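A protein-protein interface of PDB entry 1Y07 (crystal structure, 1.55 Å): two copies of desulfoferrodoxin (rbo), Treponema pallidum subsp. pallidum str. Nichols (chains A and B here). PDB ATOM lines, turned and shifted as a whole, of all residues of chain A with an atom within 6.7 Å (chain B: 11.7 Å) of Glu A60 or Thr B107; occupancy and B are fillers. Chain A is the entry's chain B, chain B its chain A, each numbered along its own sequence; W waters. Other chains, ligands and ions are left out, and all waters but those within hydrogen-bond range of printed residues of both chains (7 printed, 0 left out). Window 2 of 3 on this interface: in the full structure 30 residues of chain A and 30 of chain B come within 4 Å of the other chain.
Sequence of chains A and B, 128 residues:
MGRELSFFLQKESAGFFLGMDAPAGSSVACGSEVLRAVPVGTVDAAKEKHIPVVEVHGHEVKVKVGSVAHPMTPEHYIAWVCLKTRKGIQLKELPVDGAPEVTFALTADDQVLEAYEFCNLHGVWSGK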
ATOM      1  N   GLU A  55      -9.804   7.483  -8.319  1.00  0.00           N
ATOM      2  CA  GLU A  55      -9.003   8.692  -8.535  1.00  0.00           C
ATOM      3  C   GLU A  55      -9.958   9.857  -8.718  1.00  0.00           C
ATOM      4  O   GLU A  55     -10.654   9.935  -9.721  1.00  0.00           O
ATOM      5  CB  GLU A  55      -8.131   8.556  -9.771  1.00  0.00           C
ATOM      6  CG  GLU A  55      -7.044   7.504  -9.660  1.00  0.00           C
ATOM      7  CD  GLU A  55      -6.164   7.438 -10.889  1.00  0.00           C
ATOM      8  OE1 GLU A  55      -6.498   8.069 -11.932  1.00  0.00           O
ATOM      9  OE2 GLU A  55      -5.121   6.746 -10.805  1.00  0.00           O
ATOM     10  N   VAL A  56     -10.008  10.729  -7.722  1.00  0.00           N
ATOM     11  CA  VAL A  56     -10.904  11.863  -7.734  1.00  0.00           C
ATOM     12  C   VAL A  56     -10.190  13.097  -8.223  1.00  0.00           C
ATOM     13  O   VAL A  56      -9.015  13.393  -7.864  1.00  0.00           O
ATOM     14  CB  VAL A  56     -11.478  12.153  -6.347  1.00  0.00           C
ATOM     15  CG1 VAL A  56     -12.471  13.336  -6.396  1.00  0.00           C
ATOM     16  CG2 VAL A  56     -12.118  10.932  -5.773  1.00  0.00           C
ATOM     17  N   HIS A  57     -10.880  13.826  -9.068  1.00  0.00           N
ATOM     18  CA  HIS A  57     -10.512  15.156  -9.374  1.00  0.00           C
ATOM     19  C   HIS A  57     -11.801  15.951  -9.387  1.00  0.00           C
ATOM     20  O   HIS A  57     -12.589  15.789 -10.291  1.00  0.00           O
ATOM     21  CB  HIS A  57      -9.843  15.154 -10.705  1.00  0.00           C
ATOM     22  CG  HIS A  57     -10.249  16.277 -11.608  1.00  0.00           C
ATOM     23  ND1 HIS A  57     -10.996  16.050 -12.745  1.00  0.00           N
ATOM     24  CD2 HIS A  57      -9.914  17.606 -11.624  1.00  0.00           C
ATOM     25  CE1 HIS A  57     -11.170  17.192 -13.380  1.00  0.00           C
ATOM     26  NE2 HIS A  57     -10.527  18.157 -12.724  1.00  0.00           N
ATOM     27  N   GLY A  58     -11.943  16.848  -8.418  1.00  0.00           N
ATOM     28  CA  GLY A  58     -13.119  17.698  -8.372  1.00  0.00           C
ATOM     29  C   GLY A  58     -14.323  16.885  -8.192  1.00  0.00           C
ATOM     30  O   GLY A  58     -14.376  16.110  -7.300  1.00  0.00           O
ATOM     31  N   HIS A  59     -15.230  17.014  -9.135  1.00  0.00           N
ATOM     32  CA  HIS A  59     -16.539  16.410  -8.984  1.00  0.00           C
ATOM     33  C   HIS A  59     -16.558  15.206  -9.916  1.00  0.00           C
ATOM     34  O   HIS A  59     -17.640  14.691 -10.164  1.00  0.00           O
ATOM     35  CB  HIS A  59     -17.650  17.476  -9.249  1.00  0.00           C
ATOM     36  CG  HIS A  59     -17.665  18.607  -8.229  1.00  0.00           C
ATOM     37  ND1 HIS A  59     -18.213  19.851  -8.485  1.00  0.00           N
ATOM     38  CD2 HIS A  59     -17.112  18.701  -6.988  1.00  0.00           C
ATOM     39  CE1 HIS A  59     -18.032  20.643  -7.434  1.00  0.00           C
ATOM     40  NE2 HIS A  59     -17.376  19.966  -6.504  1.00  0.00           N
ATOM     41  N   GLU A  60     -15.423  14.730 -10.436  1.00  0.00           N
ATOM     42  CA  GLU A  60     -15.333  13.501 -11.208  1.00  0.00           C
ATOM     43  C   GLU A  60     -14.491  12.445 -10.483  1.00  0.00           C
ATOM     44  O   GLU A  60     -13.478  12.732  -9.814  1.00  0.00           O
ATOM     45  CB  GLU A  60     -14.782  13.767 -12.624  1.00  0.00           C
ATOM     46  CG  GLU A  60     -15.849  14.477 -13.460  1.00  0.00           C
ATOM     47  CD  GLU A  60     -15.640  14.475 -14.988  1.00  0.00           C
ATOM     48  OE1 GLU A  60     -14.471  14.674 -15.428  1.00  0.00           O
ATOM     49  OE2 GLU A  60     -16.671  14.355 -15.759  1.00  0.00           O
ATOM     50  N   VAL A  61     -14.903  11.198 -10.675  1.00  0.00           N
ATOM     51  CA  VAL A  61     -14.297  10.045 -10.010  1.00  0.00           C
ATOM     52  C   VAL A  61     -14.031   9.044 -11.093  1.00  0.00           C
ATOM     53  O   VAL A  61     -14.975   8.537 -11.719  1.00  0.00           O
ATOM     54  CB  VAL A  61     -15.282   9.418  -9.000  1.00  0.00           C
ATOM     55  CG1 VAL A  61     -14.700   8.114  -8.415  1.00  0.00           C
ATOM     56  CG2 VAL A  61     -15.675  10.398  -7.893  1.00  0.00           C
ATOM     57  N   LYS A  62     -12.768   8.753 -11.355  1.00  0.00           N
ATOM     58  CA  LYS A  62     -12.381   7.764 -12.341  1.00  0.00           C
ATOM     59  C   LYS A  62     -12.119   6.491 -11.590  1.00  0.00           C
ATOM     60  O   LYS A  62     -11.440   6.509 -10.552  1.00  0.00           O
ATOM     61  CB  LYS A  62     -11.127   8.207 -13.070  1.00  0.00           C
ATOM     62  CG  LYS A  62     -10.676   7.337 -14.249  1.00  0.00           C
ATOM     63  CD  LYS A  62      -9.272   7.749 -14.697  1.00  0.00           C
ATOM     64  CE  LYS A  62      -9.251   8.345 -16.105  1.00  0.00           C
ATOM     65  NZ  LYS A  62      -7.893   8.153 -16.733  1.00  0.00           N
ATOM     66  N   LYS A  92     -22.364   2.032 -14.017  1.00  0.00           N
ATOM     67  CA  LYS A  92     -22.154   2.100 -15.457  1.00  0.00           C
ATOM     68  C   LYS A  92     -21.563   0.807 -15.954  1.00  0.00           C
ATOM     69  O   LYS A  92     -20.579   0.288 -15.402  1.00  0.00           O
ATOM     70  CB  LYS A  92     -21.150   3.252 -15.799  1.00  0.00           C
ATOM     71  CG  LYS A  92     -21.705   4.652 -15.568  1.00  0.00           C
ATOM     72  CD  LYS A  92     -20.740   5.774 -15.969  1.00  0.00           C
ATOM     73  CE  LYS A  92     -21.426   7.101 -16.178  1.00  0.00           C
ATOM     74  NZ  LYS A  92     -20.556   8.105 -16.680  1.00  0.00           N
ATOM     75  N   THR A 103     -15.618   6.725 -15.688  1.00  0.00           N
ATOM     76  CA  THR A 103     -15.663   7.876 -14.853  1.00  0.00           C
ATOM     77  C   THR A 103     -17.127   8.192 -14.506  1.00  0.00           C
ATOM     78  O   THR A 103     -18.038   8.012 -15.323  1.00  0.00           O
ATOM     79  CB  THR A 103     -15.097   9.036 -15.592  1.00  0.00           C
ATOM     80  OG1 THR A 103     -13.731   8.710 -15.930  1.00  0.00           O
ATOM     81  CG2 THR A 103     -15.039  10.335 -14.698  1.00  0.00           C
ATOM     82  N   PHE A 104     -17.322   8.651 -13.292  1.00  0.00           N
ATOM     83  CA  PHE A 104     -18.598   9.084 -12.790  1.00  0.00           C
ATOM     84  C   PHE A 104     -18.465  10.553 -12.436  1.00  0.00           C
ATOM     85  O   PHE A 104     -17.380  10.983 -12.060  1.00  0.00           O
ATOM     86  CB  PHE A 104     -18.893   8.328 -11.522  1.00  0.00           C
ATOM     87  CG  PHE A 104     -19.004   6.837 -11.731  1.00  0.00           C
ATOM     88  CD1 PHE A 104     -17.896   6.023 -11.575  1.00  0.00           C
ATOM     89  CD2 PHE A 104     -20.203   6.263 -12.049  1.00  0.00           C
ATOM     90  CE1 PHE A 104     -17.969   4.629 -11.763  1.00  0.00           C
ATOM     91  CE2 PHE A 104     -20.284   4.855 -12.211  1.00  0.00           C
ATOM     92  CZ  PHE A 104     -19.164   4.070 -12.089  1.00  0.00           C
ATOM     93  N   ALA A 105     -19.564  11.294 -12.487  1.00  0.00           N
ATOM     94  CA  ALA A 105     -19.632  12.665 -12.003  1.00  0.00           C
ATOM     95  C   ALA A 105     -20.492  12.822 -10.764  1.00  0.00           C
ATOM     96  O   ALA A 105     -21.547  12.120 -10.646  1.00  0.00           O
ATOM     97  CB  ALA A 105     -20.175  13.536 -13.131  1.00  0.00           C
ATOM     98  N   LEU A 106     -20.072  13.697  -9.841  1.00  0.00           N
ATOM     99  CA  LEU A 106     -20.726  13.967  -8.577  1.00  0.00           C
ATOM    100  C   LEU A 106     -21.170  15.411  -8.538  1.00  0.00           C
ATOM    101  O   LEU A 106     -20.546  16.279  -9.155  1.00  0.00           O
ATOM    102  CB  LEU A 106     -19.757  13.608  -7.396  1.00  0.00           C
ATOM    103  CG  LEU A 106     -19.726  12.120  -6.948  1.00  0.00           C
ATOM    104  CD1 LEU A 106     -19.307  11.151  -8.082  1.00  0.00           C
ATOM    105  CD2 LEU A 106     -18.842  11.925  -5.691  1.00  0.00           C
ATOM    106  N   VAL B  56     -32.050  20.008 -17.474  1.00  0.00           N
ATOM    107  CA  VAL B  56     -30.608  19.807 -17.693  1.00  0.00           C
ATOM    108  C   VAL B  56     -29.948  21.150 -17.697  1.00  0.00           C
ATOM    109  O   VAL B  56     -30.383  22.040 -18.386  1.00  0.00           O
ATOM    110  CB  VAL B  56     -30.295  19.053 -19.011  1.00  0.00           C
ATOM    111  CG1 VAL B  56     -28.842  18.914 -19.167  1.00  0.00           C
ATOM    112  CG2 VAL B  56     -30.997  17.661 -18.980  1.00  0.00           C
ATOM    113  N   HIS B  57     -28.913  21.302 -16.871  1.00  0.00           N
ATOM    114  CA  HIS B  57     -28.073  22.472 -16.891  1.00  0.00           C
ATOM    115  C   HIS B  57     -26.608  22.070 -16.952  1.00  0.00           C
ATOM    116  O   HIS B  57     -25.971  21.745 -15.950  1.00  0.00           O
ATOM    117  CB  HIS B  57     -28.351  23.415 -15.708  1.00  0.00           C
ATOM    118  CG  HIS B  57     -29.580  24.261 -15.930  1.00  0.00           C
ATOM    119  ND1 HIS B  57     -30.815  23.881 -15.468  1.00  0.00           N
ATOM    120  CD2 HIS B  57     -29.782  25.377 -16.673  1.00  0.00           C
ATOM    121  CE1 HIS B  57     -31.722  24.758 -15.860  1.00  0.00           C
ATOM    122  NE2 HIS B  57     -31.122  25.679 -16.589  1.00  0.00           N
ATOM    123  N   GLY B  58     -26.083  22.172 -18.135  1.00  0.00           N
ATOM    124  CA  GLY B  58     -24.786  21.676 -18.453  1.00  0.00           C
ATOM    125  C   GLY B  58     -24.649  20.208 -18.154  1.00  0.00           C
ATOM    126  O   GLY B  58     -25.359  19.415 -18.726  1.00  0.00           O
ATOM    127  N   HIS B  59     -23.785  19.874 -17.188  1.00  0.00           N
ATOM    128  CA  HIS B  59     -23.573  18.475 -16.814  1.00  0.00           C
ATOM    129  C   HIS B  59     -24.432  18.051 -15.621  1.00  0.00           C
ATOM    130  O   HIS B  59     -24.335  16.916 -15.157  1.00  0.00           O
ATOM    131  CB  HIS B  59     -22.121  18.276 -16.466  1.00  0.00           C
ATOM    132  CG  HIS B  59     -21.732  18.774 -15.107  1.00  0.00           C
ATOM    133  ND1 HIS B  59     -20.693  19.649 -14.922  1.00  0.00           N
ATOM    134  CD2 HIS B  59     -22.198  18.487 -13.861  1.00  0.00           C
ATOM    135  CE1 HIS B  59     -20.526  19.873 -13.626  1.00  0.00           C
ATOM    136  NE2 HIS B  59     -21.433  19.194 -12.961  1.00  0.00           N
ATOM    137  N   GLU B  60     -25.252  18.937 -15.103  1.00  0.00           N
ATOM    138  CA  GLU B  60     -26.190  18.613 -14.048  1.00  0.00           C
ATOM    139  C   GLU B  60     -27.613  18.465 -14.535  1.00  0.00           C
ATOM    140  O   GLU B  60     -28.075  19.079 -15.469  1.00  0.00           O
ATOM    141  CB  GLU B  60     -26.087  19.620 -12.924  1.00  0.00           C
ATOM    142  CG  GLU B  60     -24.720  19.517 -12.233  1.00  0.00           C
ATOM    143  CD  GLU B  60     -24.618  20.261 -10.914  1.00  0.00           C
ATOM    144  OE1 GLU B  60     -25.256  21.302 -10.760  1.00  0.00           O
ATOM    145  OE2 GLU B  60     -23.859  19.804 -10.039  1.00  0.00           O
ATOM    146  N   VAL B  61     -28.282  17.476 -13.922  1.00  0.00           N
ATOM    147  CA  VAL B  61     -29.693  17.147 -14.200  1.00  0.00           C
ATOM    148  C   VAL B  61     -30.436  17.261 -12.909  1.00  0.00           C
ATOM    149  O   VAL B  61     -30.138  16.535 -11.967  1.00  0.00           O
ATOM    150  CB  VAL B  61     -29.840  15.744 -14.757  1.00  0.00           C
ATOM    151  CG1 VAL B  61     -31.337  15.438 -14.994  1.00  0.00           C
ATOM    152  CG2 VAL B  61     -29.056  15.562 -16.034  1.00  0.00           C
ATOM    153  N   LEU B  83     -32.247   7.999 -11.875  1.00  0.00           N
ATOM    154  CA  LEU B  83     -32.035   8.501 -13.185  1.00  0.00           C
ATOM    155  C   LEU B  83     -31.395   7.423 -14.081  1.00  0.00           C
ATOM    156  O   LEU B  83     -30.464   6.754 -13.691  1.00  0.00           O
ATOM    157  CB  LEU B  83     -31.102   9.730 -13.035  1.00  0.00           C
ATOM    158  CG  LEU B  83     -31.119  10.708 -14.139  1.00  0.00           C
ATOM    159  CD1 LEU B  83     -32.438  11.453 -14.055  1.00  0.00           C
ATOM    160  CD2 LEU B  83     -29.966  11.674 -14.031  1.00  0.00           C
ATOM    161  N   LYS B  84     -31.973   7.230 -15.254  1.00  0.00           N
ATOM    162  CA  LYS B  84     -31.431   6.439 -16.319  1.00  0.00           C
ATOM    163  C   LYS B  84     -30.802   7.390 -17.326  1.00  0.00           C
ATOM    164  O   LYS B  84     -31.461   8.292 -17.797  1.00  0.00           O
ATOM    165  CB  LYS B  84     -32.509   5.615 -16.993  1.00  0.00           C
ATOM    166  CG  LYS B  84     -31.992   4.676 -18.021  1.00  0.00           C
ATOM    167  CD  LYS B  84     -33.182   3.885 -18.522  1.00  0.00           C
ATOM    168  CE  LYS B  84     -32.885   2.966 -19.612  1.00  0.00           C
ATOM    169  NZ  LYS B  84     -34.237   2.335 -19.912  1.00  0.00           N
ATOM    170  N   THR B  85     -29.571   7.117 -17.697  1.00  0.00           N
ATOM    171  CA  THR B  85     -28.861   7.907 -18.674  1.00  0.00           C
ATOM    172  C   THR B  85     -28.364   6.971 -19.749  1.00  0.00           C
ATOM    173  O   THR B  85     -28.448   5.755 -19.627  1.00  0.00           O
ATOM    174  CB  THR B  85     -27.629   8.740 -18.054  1.00  0.00           C
ATOM    175  OG1 THR B  85     -26.594   7.848 -17.624  1.00  0.00           O
ATOM    176  CG2 THR B  85     -28.040   9.534 -16.768  1.00  0.00           C
ATOM    177  N   ARG B  86     -27.816   7.531 -20.816  1.00  0.00           N
ATOM    178  CA  ARG B  86     -27.259   6.721 -21.852  1.00  0.00           C
ATOM    179  C   ARG B  86     -26.183   5.762 -21.324  1.00  0.00           C
ATOM    180  O   ARG B  86     -26.060   4.615 -21.810  1.00  0.00           O
ATOM    181  CB  ARG B  86     -26.721   7.587 -22.967  1.00  0.00           C
ATOM    182  CG  ARG B  86     -27.759   8.250 -23.756  1.00  0.00           C
ATOM    183  CD  ARG B  86     -27.217   8.903 -25.003  1.00  0.00           C
ATOM    184  NE  ARG B  86     -28.230   9.659 -25.696  1.00  0.00           N
ATOM    185  CZ  ARG B  86     -29.143   9.192 -26.515  1.00  0.00           C
ATOM    186  NH1 ARG B  86     -29.271   7.880 -26.742  1.00  0.00           N
ATOM    187  NH2 ARG B  86     -30.003  10.050 -27.063  1.00  0.00           N
ATOM    188  N   LYS B  87     -25.373   6.248 -20.378  1.00  0.00           N
ATOM    189  CA  LYS B  87     -24.186   5.528 -19.953  1.00  0.00           C
ATOM    190  C   LYS B  87     -24.385   4.755 -18.689  1.00  0.00           C
ATOM    191  O   LYS B  87     -23.542   3.931 -18.381  1.00  0.00           O
ATOM    192  CB  LYS B  87     -22.965   6.460 -19.816  1.00  0.00           C
ATOM    193  CG  LYS B  87     -22.620   7.095 -21.165  1.00  0.00           C
ATOM    194  CD  LYS B  87     -22.228   6.173 -22.275  1.00  0.00           C
ATOM    195  CE  LYS B  87     -21.829   6.917 -23.524  1.00  0.00           C
ATOM    196  NZ  LYS B  87     -20.435   7.202 -23.465  1.00  0.00           N
ATOM    197  N   GLY B  88     -25.473   4.970 -17.967  1.00  0.00           N
ATOM    198  CA  GLY B  88     -25.608   4.311 -16.688  1.00  0.00           C
ATOM    199  C   GLY B  88     -26.876   4.666 -15.940  1.00  0.00           C
ATOM    200  O   GLY B  88     -27.826   5.139 -16.521  1.00  0.00           O
ATOM    201  N   ILE B  89     -26.862   4.369 -14.650  1.00  0.00           N
ATOM    202  CA  ILE B  89     -27.962   4.602 -13.756  1.00  0.00           C
ATOM    203  C   ILE B  89     -27.447   5.323 -12.490  1.00  0.00           C
ATOM    204  O   ILE B  89     -26.277   5.186 -12.102  1.00  0.00           O
ATOM    205  CB  ILE B  89     -28.775   3.320 -13.411  1.00  0.00           C
ATOM    206  CG1 ILE B  89     -27.947   2.291 -12.659  1.00  0.00           C
ATOM    207  CG2 ILE B  89     -29.388   2.755 -14.672  1.00  0.00           C
ATOM    208  CD1 ILE B  89     -28.843   1.247 -12.021  1.00  0.00           C
ATOM    209  N   GLN B  90     -28.339   6.097 -11.896  1.00  0.00           N
ATOM    210  CA  GLN B  90     -28.134   6.721 -10.608  1.00  0.00           C
ATOM    211  C   GLN B  90     -29.356   6.666  -9.736  1.00  0.00           C
ATOM    212  O   GLN B  90     -30.459   6.681 -10.218  1.00  0.00           O
ATOM    213  CB  GLN B  90     -27.725   8.227 -10.812  1.00  0.00           C
ATOM    214  CG  GLN B  90     -26.528   8.399 -11.682  1.00  0.00           C
ATOM    215  CD  GLN B  90     -25.915   9.752 -11.486  1.00  0.00           C
ATOM    216  OE1 GLN B  90     -25.703  10.215 -10.372  1.00  0.00           O
ATOM    217  NE2 GLN B  90     -25.549  10.437 -12.622  1.00  0.00           N
ATOM    218  N   THR B 103     -30.496  16.764  -7.535  1.00  0.00           N
ATOM    219  CA  THR B 103     -29.630  16.925  -8.694  1.00  0.00           C
ATOM    220  C   THR B 103     -28.618  15.781  -8.819  1.00  0.00           C
ATOM    221  O   THR B 103     -28.093  15.255  -7.824  1.00  0.00           O
ATOM    222  CB  THR B 103     -28.933  18.282  -8.618  1.00  0.00           C
ATOM    223  OG1 THR B 103     -29.947  19.283  -8.607  1.00  0.00           O
ATOM    224  CG2 THR B 103     -28.167  18.616  -9.830  1.00  0.00           C
ATOM    225  N   PHE B 104     -28.395  15.387 -10.069  1.00  0.00           N
ATOM    226  CA  PHE B 104     -27.400  14.422 -10.441  1.00  0.00           C
ATOM    227  C   PHE B 104     -26.381  15.098 -11.362  1.00  0.00           C
ATOM    228  O   PHE B 104     -26.685  16.051 -12.089  1.00  0.00           O
ATOM    229  CB  PHE B 104     -28.029  13.292 -11.223  1.00  0.00           C
ATOM    230  CG  PHE B 104     -29.130  12.600 -10.464  1.00  0.00           C
ATOM    231  CD1 PHE B 104     -30.467  13.053 -10.509  1.00  0.00           C
ATOM    232  CD2 PHE B 104     -28.859  11.459  -9.707  1.00  0.00           C
ATOM    233  CE1 PHE B 104     -31.451  12.448  -9.804  1.00  0.00           C
ATOM    234  CE2 PHE B 104     -29.877  10.803  -9.050  1.00  0.00           C
ATOM    235  CZ  PHE B 104     -31.181  11.255  -9.083  1.00  0.00           C
ATOM    236  N   ALA B 105     -25.182  14.563 -11.365  1.00  0.00           N
ATOM    237  CA  ALA B 105     -24.132  14.994 -12.287  1.00  0.00           C
ATOM    238  C   ALA B 105     -23.748  13.902 -13.266  1.00  0.00           C
ATOM    239  O   ALA B 105     -23.734  12.730 -12.931  1.00  0.00           O
ATOM    240  CB  ALA B 105     -22.877  15.482 -11.494  1.00  0.00           C
ATOM    241  N   LEU B 106     -23.565  14.338 -14.524  1.00  0.00           N
ATOM    242  CA  LEU B 106     -23.172  13.499 -15.647  1.00  0.00           C
ATOM    243  C   LEU B 106     -21.835  13.822 -16.175  1.00  0.00           C
ATOM    244  O   LEU B 106     -21.397  14.995 -16.156  1.00  0.00           O
ATOM    245  CB  LEU B 106     -24.186  13.589 -16.799  1.00  0.00           C
ATOM    246  CG  LEU B 106     -25.512  12.828 -16.646  1.00  0.00           C
ATOM    247  CD1 LEU B 106     -26.334  13.006 -15.411  1.00  0.00           C
ATOM    248  CD2 LEU B 106     -26.363  13.160 -17.881  1.00  0.00           C
ATOM    249  N   THR B 107     -21.163  12.812 -16.697  1.00  0.00           N
ATOM    250  CA  THR B 107     -19.929  13.013 -17.494  1.00  0.00           C
ATOM    251  C   THR B 107     -20.276  13.597 -18.843  1.00  0.00           C
ATOM    252  O   THR B 107     -21.445  13.545 -19.293  1.00  0.00           O
ATOM    253  CB  THR B 107     -19.146  11.721 -17.635  1.00  0.00           C
ATOM    254  OG1 THR B 107     -19.967  10.698 -18.206  1.00  0.00           O
ATOM    255  CG2 THR B 107     -18.672  11.266 -16.257  1.00  0.00           C
ATOM    256  N   ALA B 108     -19.260  14.206 -19.515  1.00  0.00           N
ATOM    257  CA  ALA B 108     -19.615  14.896 -20.729  1.00  0.00           C
ATOM    258  C   ALA B 108     -20.117  14.053 -21.889  1.00  0.00           C
ATOM    259  O   ALA B 108     -20.830  14.536 -22.792  1.00  0.00           O
ATOM    260  CB  ALA B 108     -18.335  15.642 -21.221  1.00  0.00           C
ATOM    261  N   ASP B 109     -19.790  12.766 -21.842  1.00  0.00           N
ATOM    262  CA  ASP B 109     -20.199  11.755 -22.843  1.00  0.00           C
ATOM    263  C   ASP B 109     -21.597  11.188 -22.591  1.00  0.00           C
ATOM    264  O   ASP B 109     -22.104  10.475 -23.406  1.00  0.00           O
ATOM    265  CB  ASP B 109     -19.156  10.628 -22.822  1.00  0.00           C
ATOM    266  CG  ASP B 109     -19.117   9.917 -21.481  1.00  0.00           C
ATOM    267  OD1 ASP B 109     -18.792  10.540 -20.454  1.00  0.00           O
ATOM    268  OD2 ASP B 109     -19.427   8.751 -21.384  1.00  0.00           O
ATOM    269  N   ASP B 110     -22.197  11.583 -21.489  1.00  0.00           N
ATOM    270  CA  ASP B 110     -23.486  11.057 -21.092  1.00  0.00           C
ATOM    271  C   ASP B 110     -24.638  12.012 -21.407  1.00  0.00           C
ATOM    272  O   ASP B 110     -24.422  13.214 -21.748  1.00  0.00           O
ATOM    273  CB  ASP B 110     -23.388  10.767 -19.624  1.00  0.00           C
ATOM    274  CG  ASP B 110     -24.361   9.644 -19.196  1.00  0.00           C
ATOM    275  OD1 ASP B 110     -25.138   9.148 -20.065  1.00  0.00           O
ATOM    276  OD2 ASP B 110     -24.423   9.209 -18.004  1.00  0.00           O
ATOM    277  N   GLN B 111     -25.850  11.488 -21.349  1.00  0.00           N
ATOM    278  CA  GLN B 111     -27.060  12.245 -21.573  1.00  0.00           C
ATOM    279  C   GLN B 111     -28.163  11.588 -20.827  1.00  0.00           C
ATOM    280  O   GLN B 111     -28.298  10.354 -20.852  1.00  0.00           O
ATOM    281  CB  GLN B 111     -27.394  12.324 -23.064  1.00  0.00           C
ATOM    282  CG  GLN B 111     -28.682  13.044 -23.356  1.00  0.00           C
ATOM    283  CD  GLN B 111     -28.882  13.332 -24.842  1.00  0.00           C
ATOM    284  OE1 GLN B 111     -28.632  12.471 -25.704  1.00  0.00           O
ATOM    285  NE2 GLN B 111     -29.314  14.570 -25.147  1.00  0.00           N
ATOM    286  N   VAL B 112     -29.026  12.392 -20.207  1.00  0.00           N
ATOM    287  CA  VAL B 112     -30.182  11.862 -19.532  1.00  0.00           C
ATOM    288  C   VAL B 112     -31.195  11.171 -20.470  1.00  0.00           C
ATOM    289  O   VAL B 112     -31.383  11.592 -21.613  1.00  0.00           O
ATOM    290  CB  VAL B 112     -30.921  12.935 -18.684  1.00  0.00           C
ATOM    291  CG1 VAL B 112     -31.637  13.945 -19.531  1.00  0.00           C
ATOM    292  CG2 VAL B 112     -31.871  12.262 -17.715  1.00  0.00           C
ATOM    293  N   LEU B 113     -31.835  10.131 -19.993  1.00  0.00           N
ATOM    294  CA  LEU B 113     -32.931   9.449 -20.706  1.00  0.00           C
ATOM    295  C   LEU B 113     -34.259   9.577 -19.969  1.00  0.00           C
ATOM    296  O   LEU B 113     -35.224  10.066 -20.569  1.00  0.00           O
ATOM    297  CB  LEU B 113     -32.616   8.003 -21.021  1.00  0.00           C
ATOM    298  CG  LEU B 113     -31.454   7.723 -21.965  1.00  0.00           C
ATOM    299  CD1 LEU B 113     -31.166   6.233 -22.150  1.00  0.00           C
ATOM    300  CD2 LEU B 113     -31.723   8.351 -23.351  1.00  0.00           C
HETATM  301  O   HOH W   1     -18.954  16.156 -15.501  1.00  0.00           O
HETATM  302  O   HOH W   2     -24.155  12.404  -9.680  1.00  0.00           O
HETATM  303  O   HOH W   3     -20.848  18.446 -10.619  1.00  0.00           O
HETATM  304  O   HOH W   4     -19.343   7.411 -19.108  1.00  0.00           O
HETATM  305  O   HOH W   5     -22.231  10.402 -13.437  1.00  0.00           O
HETATM  306  O   HOH W   6     -16.702  14.455 -18.261  1.00  0.00           O
HETATM  307  O   HOH W   7     -22.502  10.184 -16.230  1.00  0.00           O
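OG1 of Thr B107 is in hydrogen-bond range of NZ of Lys A92 (3.1 Å). O of Ala B105 sits close to O of Ala A105 (3.2 Å).
O of His B59 lies within hydrogen-bond range of N of Leu B106 (2.8 Å). The side-chain hydroxyl (OG1) of Thr B85 sits close to the backbone NH (N) of Lys B87 (3.4 Å). OD1 of Asp B110 sits at hydrogen-bond distance from N of Lys B87 (2.9 Å). NE2 of Gln B90 is in hydrogen-bond range of O of Ala B105 (2.9 Å). The backbone NH (N) of Phe A104 sits at hydrogen-bond distance from the backbone carbonyl oxygen (O) of Val A61 (2.8 Å). NZ of Lys A92 lies within hydrogen-bond range of O of Thr A103 (2.9 Å).
Among the printed residues, pairs that only touch across the chains: Glu A60 with Thr B107 (3.7 Å), Lys A92 with Lys B87 (3.4 Å), Thr A103 with Thr B107 (3.4 Å), Phe A104 with Thr B107 (3.9 Å), Ala A105 with Leu B106 (3.5 Å), Ala A105 with Thr B107 (3.8 Å) and Leu A106 with Ala B105 (3.4 Å).
Thr B107 touches five residues of chain A. Gly A58 touches none of the printed residues of chain B. His A59 touches none of the printed residues of chain B. No residue of chain B comes within 4 Å of Val A61. Thr A103 touches just one residue of chain B: Thr B107. Ala A105 touches just these residues of chain B: Ala B105 (3.2 Å), Leu B106 (3.5 Å) and Thr B107 (3.8 Å). Of the printed residues of chain B, Leu A106 touches Ala B105. Of the printed residues of chain A, Ala B105 touches Ala A105 and Leu A106. Printed residues of chain A within 4 Å of Leu B106: Ala A105. Of the printed residues of chain B, Lys A92 touches Lys B87 and Thr B107. Of the printed residues of chain B, Phe A104 touches Thr B107. Of the printed residues of chain A, Lys B87 touches Lys A92. Asp B110 touches none of the printed residues of chain A. His B57 touches none of the printed residues of chain A. The nearest residue of chain A that does not touch Thr B107 is Val A61 (6.5 Å).
Hydrophobic or aromatic side chains of chain B that line the printed part of chain A: Ala B105. Among the printed residues, 9 pairs touch across the chains.
Ala B105 touches its own counterpart, Ala A105. Ala A105 touches Leu B106, and with the chains exchanged Leu A106 touches Ala B105. 10 positions are printed for both chains.
Water W3 lies within hydrogen-bond range of a ring nitrogen (NE2) of His B59 (2.5 Å), the backbone carbonyl oxygen of Leu A106 (2.6 Å) and the side-chain carboxylate of Glu B60 (3.4 Å). Water W4 lies within hydrogen-bond range of OD2 of Asp B109 (2.6 Å), NZ of Lys A92 (2.8 Å) and OG1 of Thr B107 (3.5 Å). Water W1 lies within hydrogen-bond range of the backbone carbonyl oxygen (O) of Leu B106 (2.8 Å) and the side-chain carboxylate (OE2) of Glu A60 (2.9 Å). Water W5 lies within hydrogen-bond range of O of Ala B105 (2.8 Å), N of Ala A105 (3.0 Å) and NE2 of Gln B90 (3.4 Å).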
